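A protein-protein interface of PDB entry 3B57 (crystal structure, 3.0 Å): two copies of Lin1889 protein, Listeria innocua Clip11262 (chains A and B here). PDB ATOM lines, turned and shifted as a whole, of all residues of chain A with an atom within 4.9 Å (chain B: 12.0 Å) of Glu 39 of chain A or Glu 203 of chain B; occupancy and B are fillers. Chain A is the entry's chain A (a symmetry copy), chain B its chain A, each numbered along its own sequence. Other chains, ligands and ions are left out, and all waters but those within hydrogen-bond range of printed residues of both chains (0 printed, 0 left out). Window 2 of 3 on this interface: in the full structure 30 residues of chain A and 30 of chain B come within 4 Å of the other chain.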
ATOM      1  N   LYS A  35      -9.757   1.215 -33.740  1.00  0.00           N
ATOM      2  CA  LYS A  35      -9.128  -0.079 -34.004  1.00  0.00           C
ATOM      3  C   LYS A  35      -9.963  -1.207 -33.411  1.00  0.00           C
ATOM      4  O   LYS A  35     -10.142  -2.259 -34.028  1.00  0.00           O
ATOM      5  CB  LYS A  35      -7.734  -0.153 -33.381  1.00  0.00           C
ATOM      6  CG  LYS A  35      -6.672   0.650 -34.084  1.00  0.00           C
ATOM      7  CD  LYS A  35      -5.313   0.185 -33.616  1.00  0.00           C
ATOM      8  CE  LYS A  35      -4.188   0.762 -34.458  1.00  0.00           C
ATOM      9  NZ  LYS A  35      -2.863   0.199 -34.033  1.00  0.00           N
ATOM     10  N   LEU A  36     -10.465  -0.975 -32.202  1.00  0.00           N
ATOM     11  CA  LEU A  36     -11.262  -1.959 -31.493  1.00  0.00           C
ATOM     12  C   LEU A  36     -12.561  -2.274 -32.213  1.00  0.00           C
ATOM     13  O   LEU A  36     -12.927  -3.438 -32.380  1.00  0.00           O
ATOM     14  CB  LEU A  36     -11.562  -1.453 -30.085  1.00  0.00           C
ATOM     15  CG  LEU A  36     -11.175  -2.334 -28.895  1.00  0.00           C
ATOM     16  CD1 LEU A  36      -9.910  -3.122 -29.171  1.00  0.00           C
ATOM     17  CD2 LEU A  36     -10.989  -1.415 -27.691  1.00  0.00           C
ATOM     18  N   SER A  37     -13.273  -1.240 -32.640  1.00  0.00           N
ATOM     19  CA  SER A  37     -14.520  -1.492 -33.335  1.00  0.00           C
ATOM     20  C   SER A  37     -14.212  -2.162 -34.683  1.00  0.00           C
ATOM     21  O   SER A  37     -14.974  -3.010 -35.145  1.00  0.00           O
ATOM     22  CB  SER A  37     -15.288  -0.194 -33.538  1.00  0.00           C
ATOM     23  OG  SER A  37     -14.531   0.682 -34.321  1.00  0.00           O
ATOM     24  N   LYS A  38     -13.097  -1.801 -35.311  1.00  0.00           N
ATOM     25  CA  LYS A  38     -12.749  -2.432 -36.574  1.00  0.00           C
ATOM     26  C   LYS A  38     -12.601  -3.941 -36.353  1.00  0.00           C
ATOM     27  O   LYS A  38     -13.210  -4.744 -37.069  1.00  0.00           O
ATOM     28  CB  LYS A  38     -11.452  -1.846 -37.124  1.00  0.00           C
ATOM     29  CG  LYS A  38     -11.625  -1.098 -38.447  1.00  0.00           C
ATOM     30  CD  LYS A  38     -10.484  -0.111 -38.683  1.00  0.00           C
ATOM     31  CE  LYS A  38      -9.133  -0.810 -38.676  1.00  0.00           C
ATOM     32  NZ  LYS A  38      -8.044   0.130 -38.293  1.00  0.00           N
ATOM     33  N   GLU A  39     -11.808  -4.312 -35.345  1.00  0.00           N
ATOM     34  CA  GLU A  39     -11.546  -5.716 -34.983  1.00  0.00           C
ATOM     35  C   GLU A  39     -12.836  -6.490 -34.734  1.00  0.00           C
ATOM     36  O   GLU A  39     -13.029  -7.581 -35.251  1.00  0.00           O
ATOM     37  CB  GLU A  39     -10.683  -5.770 -33.716  1.00  0.00           C
ATOM     38  CG  GLU A  39     -10.076  -7.135 -33.423  1.00  0.00           C
ATOM     39  CD  GLU A  39      -9.524  -7.260 -31.994  1.00  0.00           C
ATOM     40  OE1 GLU A  39     -10.302  -7.618 -31.079  1.00  0.00           O
ATOM     41  OE2 GLU A  39      -8.317  -6.991 -31.779  1.00  0.00           O
ATOM     42  N   ILE A  40     -13.706  -5.912 -33.924  1.00  0.00           N
ATOM     43  CA  ILE A  40     -14.968  -6.522 -33.599  1.00  0.00           C
ATOM     44  C   ILE A  40     -15.861  -6.818 -34.806  1.00  0.00           C
ATOM     45  O   ILE A  40     -16.471  -7.893 -34.895  1.00  0.00           O
ATOM     46  CB  ILE A  40     -15.737  -5.624 -32.657  1.00  0.00           C
ATOM     47  CG1 ILE A  40     -14.923  -5.443 -31.392  1.00  0.00           C
ATOM     48  CG2 ILE A  40     -17.139  -6.187 -32.408  1.00  0.00           C
ATOM     49  CD1 ILE A  40     -15.573  -4.557 -30.386  1.00  0.00           C
ATOM     50  N   GLN A  41     -15.951  -5.867 -35.737  1.00  0.00           N
ATOM     51  CA  GLN A  41     -16.824  -6.044 -36.897  1.00  0.00           C
ATOM     52  C   GLN A  41     -16.382  -7.199 -37.776  1.00  0.00           C
ATOM     53  O   GLN A  41     -17.216  -7.926 -38.325  1.00  0.00           O
ATOM     54  CB  GLN A  41     -16.909  -4.738 -37.709  1.00  0.00           C
ATOM     55  CG  GLN A  41     -16.120  -4.685 -39.021  1.00  0.00           C
ATOM     56  CD  GLN A  41     -16.818  -5.403 -40.179  1.00  0.00           C
ATOM     57  OE1 GLN A  41     -18.053  -5.386 -40.292  1.00  0.00           O
ATOM     58  NE2 GLN A  41     -16.025  -6.013 -41.058  1.00  0.00           N
ATOM     59  N   SER A  42     -15.068  -7.372 -37.889  1.00  0.00           N
ATOM     60  CA  SER A  42     -14.503  -8.442 -38.700  1.00  0.00           C
ATOM     61  C   SER A  42     -15.001  -9.811 -38.241  1.00  0.00           C
ATOM     62  O   SER A  42     -14.706 -10.828 -38.864  1.00  0.00           O
ATOM     63  CB  SER A  42     -12.980  -8.427 -38.617  1.00  0.00           C
ATOM     64  OG  SER A  42     -12.565  -9.327 -37.604  1.00  0.00           O
ATOM     65  N   LYS A  43     -15.741  -9.838 -37.143  1.00  0.00           N
ATOM     66  CA  LYS A  43     -16.258 -11.099 -36.650  1.00  0.00           C
ATOM     67  C   LYS A  43     -17.721 -10.997 -36.293  1.00  0.00           C
ATOM     68  O   LYS A  43     -18.390 -12.011 -36.098  1.00  0.00           O
ATOM     69  CB  LYS A  43     -15.468 -11.583 -35.437  1.00  0.00           C
ATOM     70  CG  LYS A  43     -14.095 -12.106 -35.776  1.00  0.00           C
ATOM     71  CD  LYS A  43     -13.528 -12.901 -34.626  1.00  0.00           C
ATOM     72  CE  LYS A  43     -12.143 -13.398 -34.978  1.00  0.00           C
ATOM     73  NZ  LYS A  43     -11.334 -12.238 -35.448  1.00  0.00           N
ATOM     74  N   THR A 176     -17.818 -11.435 -29.656  1.00  0.00           N
ATOM     75  CA  THR A 176     -16.442 -11.139 -30.011  1.00  0.00           C
ATOM     76  C   THR A 176     -15.911 -10.185 -28.960  1.00  0.00           C
ATOM     77  O   THR A 176     -14.845 -10.407 -28.386  1.00  0.00           O
ATOM     78  CB  THR A 176     -16.342 -10.506 -31.406  1.00  0.00           C
ATOM     79  OG1 THR A 176     -16.873 -11.417 -32.375  1.00  0.00           O
ATOM     80  CG2 THR A 176     -14.892 -10.206 -31.758  1.00  0.00           C
ATOM     81  N   ILE A 180     -12.623 -10.555 -26.316  1.00  0.00           N
ATOM     82  CA  ILE A 180     -11.458  -9.675 -26.296  1.00  0.00           C
ATOM     83  C   ILE A 180     -11.460  -8.905 -24.995  1.00  0.00           C
ATOM     84  O   ILE A 180     -10.628  -8.033 -24.761  1.00  0.00           O
ATOM     85  CB  ILE A 180     -11.381  -8.708 -27.504  1.00  0.00           C
ATOM     86  CG1 ILE A 180     -12.633  -7.864 -27.640  1.00  0.00           C
ATOM     87  CG2 ILE A 180     -11.183  -9.517 -28.754  1.00  0.00           C
ATOM     88  CD1 ILE A 180     -12.782  -7.267 -29.048  1.00  0.00           C
ATOM     89  N   GLN B 193       3.002  -5.616 -19.166  1.00  0.00           N
ATOM     90  CA  GLN B 193       2.857  -6.446 -20.344  1.00  0.00           C
ATOM     91  C   GLN B 193       1.467  -6.220 -20.912  1.00  0.00           C
ATOM     92  O   GLN B 193       1.321  -5.790 -22.050  1.00  0.00           O
ATOM     93  CB  GLN B 193       3.067  -7.909 -19.977  1.00  0.00           C
ATOM     94  CG  GLN B 193       4.463  -8.164 -19.455  1.00  0.00           C
ATOM     95  CD  GLN B 193       4.663  -9.584 -18.959  1.00  0.00           C
ATOM     96  OE1 GLN B 193       4.375 -10.544 -19.680  1.00  0.00           O
ATOM     97  NE2 GLN B 193       5.165  -9.728 -17.723  1.00  0.00           N
ATOM     98  N   ALA B 194       0.450  -6.465 -20.096  1.00  0.00           N
ATOM     99  CA  ALA B 194      -0.931  -6.288 -20.517  1.00  0.00           C
ATOM    100  C   ALA B 194      -1.212  -4.886 -21.060  1.00  0.00           C
ATOM    101  O   ALA B 194      -2.003  -4.734 -21.985  1.00  0.00           O
ATOM    102  CB  ALA B 194      -1.872  -6.594 -19.355  1.00  0.00           C
ATOM    103  N   LEU B 195      -0.577  -3.860 -20.500  1.00  0.00           N
ATOM    104  CA  LEU B 195      -0.828  -2.506 -20.986  1.00  0.00           C
ATOM    105  C   LEU B 195      -0.363  -2.393 -22.431  1.00  0.00           C
ATOM    106  O   LEU B 195      -1.178  -2.231 -23.336  1.00  0.00           O
ATOM    107  CB  LEU B 195      -0.101  -1.449 -20.131  1.00  0.00           C
ATOM    108  CG  LEU B 195      -0.764  -0.056 -20.012  1.00  0.00           C
ATOM    109  CD1 LEU B 195       0.258   1.018 -19.648  1.00  0.00           C
ATOM    110  CD2 LEU B 195      -1.432   0.297 -21.313  1.00  0.00           C
ATOM    111  N   GLU B 196       0.946  -2.505 -22.644  1.00  0.00           N
ATOM    112  CA  GLU B 196       1.533  -2.384 -23.982  1.00  0.00           C
ATOM    113  C   GLU B 196       0.861  -3.260 -25.023  1.00  0.00           C
ATOM    114  O   GLU B 196       0.946  -2.995 -26.223  1.00  0.00           O
ATOM    115  CB  GLU B 196       3.021  -2.712 -23.939  1.00  0.00           C
ATOM    116  CG  GLU B 196       3.814  -1.718 -23.141  1.00  0.00           C
ATOM    117  CD  GLU B 196       5.281  -2.072 -23.056  1.00  0.00           C
ATOM    118  OE1 GLU B 196       5.596  -3.268 -22.845  1.00  0.00           O
ATOM    119  OE2 GLU B 196       6.123  -1.153 -23.183  1.00  0.00           O
ATOM    120  N   LYS B 197       0.184  -4.298 -24.557  1.00  0.00           N
ATOM    121  CA  LYS B 197      -0.482  -5.203 -25.461  1.00  0.00           C
ATOM    122  C   LYS B 197      -1.835  -4.652 -25.885  1.00  0.00           C
ATOM    123  O   LYS B 197      -2.128  -4.587 -27.072  1.00  0.00           O
ATOM    124  CB  LYS B 197      -0.624  -6.568 -24.800  1.00  0.00           C
ATOM    125  CG  LYS B 197      -1.243  -7.608 -25.676  1.00  0.00           C
ATOM    126  CD  LYS B 197      -1.311  -8.929 -24.942  1.00  0.00           C
ATOM    127  CE  LYS B 197      -2.282  -9.884 -25.640  1.00  0.00           C
ATOM    128  NZ  LYS B 197      -3.647  -9.263 -25.802  1.00  0.00           N
ATOM    129  N   GLU B 198      -2.659  -4.240 -24.928  1.00  0.00           N
ATOM    130  CA  GLU B 198      -3.966  -3.705 -25.292  1.00  0.00           C
ATOM    131  C   GLU B 198      -3.880  -2.233 -25.629  1.00  0.00           C
ATOM    132  O   GLU B 198      -4.885  -1.585 -25.907  1.00  0.00           O
ATOM    133  CB  GLU B 198      -5.004  -3.944 -24.179  1.00  0.00           C
ATOM    134  CG  GLU B 198      -4.612  -3.519 -22.784  1.00  0.00           C
ATOM    135  CD  GLU B 198      -5.705  -3.821 -21.744  1.00  0.00           C
ATOM    136  OE1 GLU B 198      -6.738  -3.106 -21.729  1.00  0.00           O
ATOM    137  OE2 GLU B 198      -5.536  -4.774 -20.943  1.00  0.00           O
ATOM    138  N   LEU B 199      -2.661  -1.715 -25.645  1.00  0.00           N
ATOM    139  CA  LEU B 199      -2.452  -0.305 -25.939  1.00  0.00           C
ATOM    140  C   LEU B 199      -2.276  -0.099 -27.445  1.00  0.00           C
ATOM    141  O   LEU B 199      -2.261   1.031 -27.943  1.00  0.00           O
ATOM    142  CB  LEU B 199      -1.224   0.189 -25.167  1.00  0.00           C
ATOM    143  CG  LEU B 199      -1.110   1.679 -24.857  1.00  0.00           C
ATOM    144  CD1 LEU B 199      -2.410   2.204 -24.259  1.00  0.00           C
ATOM    145  CD2 LEU B 199       0.042   1.878 -23.900  1.00  0.00           C
ATOM    146  N   LYS B 200      -2.161  -1.214 -28.157  1.00  0.00           N
ATOM    147  CA  LYS B 200      -1.990  -1.206 -29.602  1.00  0.00           C
ATOM    148  C   LYS B 200      -3.019  -2.111 -30.277  1.00  0.00           C
ATOM    149  O   LYS B 200      -3.095  -2.178 -31.504  1.00  0.00           O
ATOM    150  CB  LYS B 200      -0.575  -1.669 -29.945  1.00  0.00           C
ATOM    151  CG  LYS B 200       0.490  -0.777 -29.332  1.00  0.00           C
ATOM    152  CD  LYS B 200       1.881  -1.160 -29.782  1.00  0.00           C
ATOM    153  CE  LYS B 200       2.206  -2.587 -29.387  1.00  0.00           C
ATOM    154  NZ  LYS B 200       3.605  -2.931 -29.760  1.00  0.00           N
ATOM    155  N   VAL B 201      -3.814  -2.789 -29.454  1.00  0.00           N
ATOM    156  CA  VAL B 201      -4.847  -3.711 -29.916  1.00  0.00           C
ATOM    157  C   VAL B 201      -4.223  -4.815 -30.760  1.00  0.00           C
ATOM    158  O   VAL B 201      -4.191  -4.718 -31.984  1.00  0.00           O
ATOM    159  CB  VAL B 201      -5.921  -2.985 -30.761  1.00  0.00           C
ATOM    160  CG1 VAL B 201      -7.078  -3.935 -31.056  1.00  0.00           C
ATOM    161  CG2 VAL B 201      -6.417  -1.743 -30.030  1.00  0.00           C
ATOM    162  N   LEU B 202      -3.728  -5.865 -30.108  1.00  0.00           N
ATOM    163  CA  LEU B 202      -3.086  -6.977 -30.816  1.00  0.00           C
ATOM    164  C   LEU B 202      -3.939  -8.244 -30.854  1.00  0.00           C
ATOM    165  O   LEU B 202      -4.232  -8.832 -29.813  1.00  0.00           O
ATOM    166  CB  LEU B 202      -1.720  -7.296 -30.176  1.00  0.00           C
ATOM    167  CG  LEU B 202      -0.531  -6.363 -30.442  1.00  0.00           C
ATOM    168  CD1 LEU B 202      -0.897  -4.932 -30.101  1.00  0.00           C
ATOM    169  CD2 LEU B 202       0.669  -6.815 -29.625  1.00  0.00           C
ATOM    170  N   GLU B 203      -4.328  -8.660 -32.061  1.00  0.00           N
ATOM    171  CA  GLU B 203      -5.144  -9.865 -32.267  1.00  0.00           C
ATOM    172  C   GLU B 203      -5.479 -10.071 -33.753  1.00  0.00           C
ATOM    173  O   GLU B 203      -6.676  -9.988 -34.115  1.00  0.00           O
ATOM    174  CB  GLU B 203      -6.447  -9.786 -31.457  1.00  0.00           C
ATOM    175  CG  GLU B 203      -6.493 -10.664 -30.198  1.00  0.00           C
ATOM    176  CD  GLU B 203      -7.797 -10.493 -29.414  1.00  0.00           C
ATOM    177  OE1 GLU B 203      -8.116  -9.341 -29.033  1.00  0.00           O
ATOM    178  OE2 GLU B 203      -8.493 -11.509 -29.174  1.00  0.00           O
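The backbone carbonyl oxygen (O) of Lys 200 of chain B lies within hydrogen-bond range of the side-chain amino group (NZ) of Lys 35 of chain A (3.5 Å). The side-chain carboxylate (OE1) of Glu 39 of chain A sits close to the side-chain carboxylate (OE1) of Glu 203 of chain B (3.5 Å).
OG of Ser 42 of chain A sits at hydrogen-bond distance from O of Glu 39 of chain A (3.0 Å).
Among the printed residues, pairs that only touch across the chains: Ile 180 of chain A with Glu 203 of chain B, Glu 39 of chain A with Val 201 of chain B, Leu 36 of chain A with Val 201 of chain B and Lys 35 of chain A with Val 201 of chain B.
Of the printed residues of chain B, Lys 35 of chain A touches Lys 200 and Val 201. Leu 36 of chain A touches just one residue of chain B: Val 201 (3.5 Å). No residue of chain B comes within 4 Å of Ser 37 of chain A. Lys 38 of chain A touches none of the printed residues of chain B. Glu 39 of chain A touches just these residues of chain B: Val 201 (3.4 Å) and Glu 203 (3.4 Å). No residue of chain B comes within 4 Å of Ile 40 of chain A. No residue of chain B comes within 4 Å of Gln 41 of chain A. No residue of chain B comes within 4 Å of Ser 42 of chain A. No residue of chain B comes within 4 Å of Lys 43 of chain A. Ile 180 of chain A touches just one residue of chain B: Glu 203. Lys 197 of chain B touches none of the printed residues of chain A. Glu 198 of chain B touches none of the printed residues of chain A. Of the printed residues of chain A, Val 201 of chain B touches Lys 35, Leu 36 and Glu 39. Glu 203 of chain B touches just these residues of chain A: Glu 39 (3.4 Å) and Ile 180 (3.1 Å). The nearest residue of chain B that does not touch Glu 39 of chain A is Leu 202 of chain B (4.6 Å). The nearest printed residue of chain A that does not touch Glu 203 of chain B is Lys 43 of chain A (5.3 Å).
Hydrophobic or aromatic side chains of chain A within 4 Å of the printed part of chain B: Leu 36 and Ile 180. Among the printed residues, 6 pairs touch across the chains. Among the printed residues, no Asp or Glu carboxylate lies within 4 Å of a Lys or Arg side-chain nitrogen of the other chain.
No position is printed for both chains. Of the 6 pairs that touch across the chains among the printed residues, none has its exchanged pair printed and touching as well.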
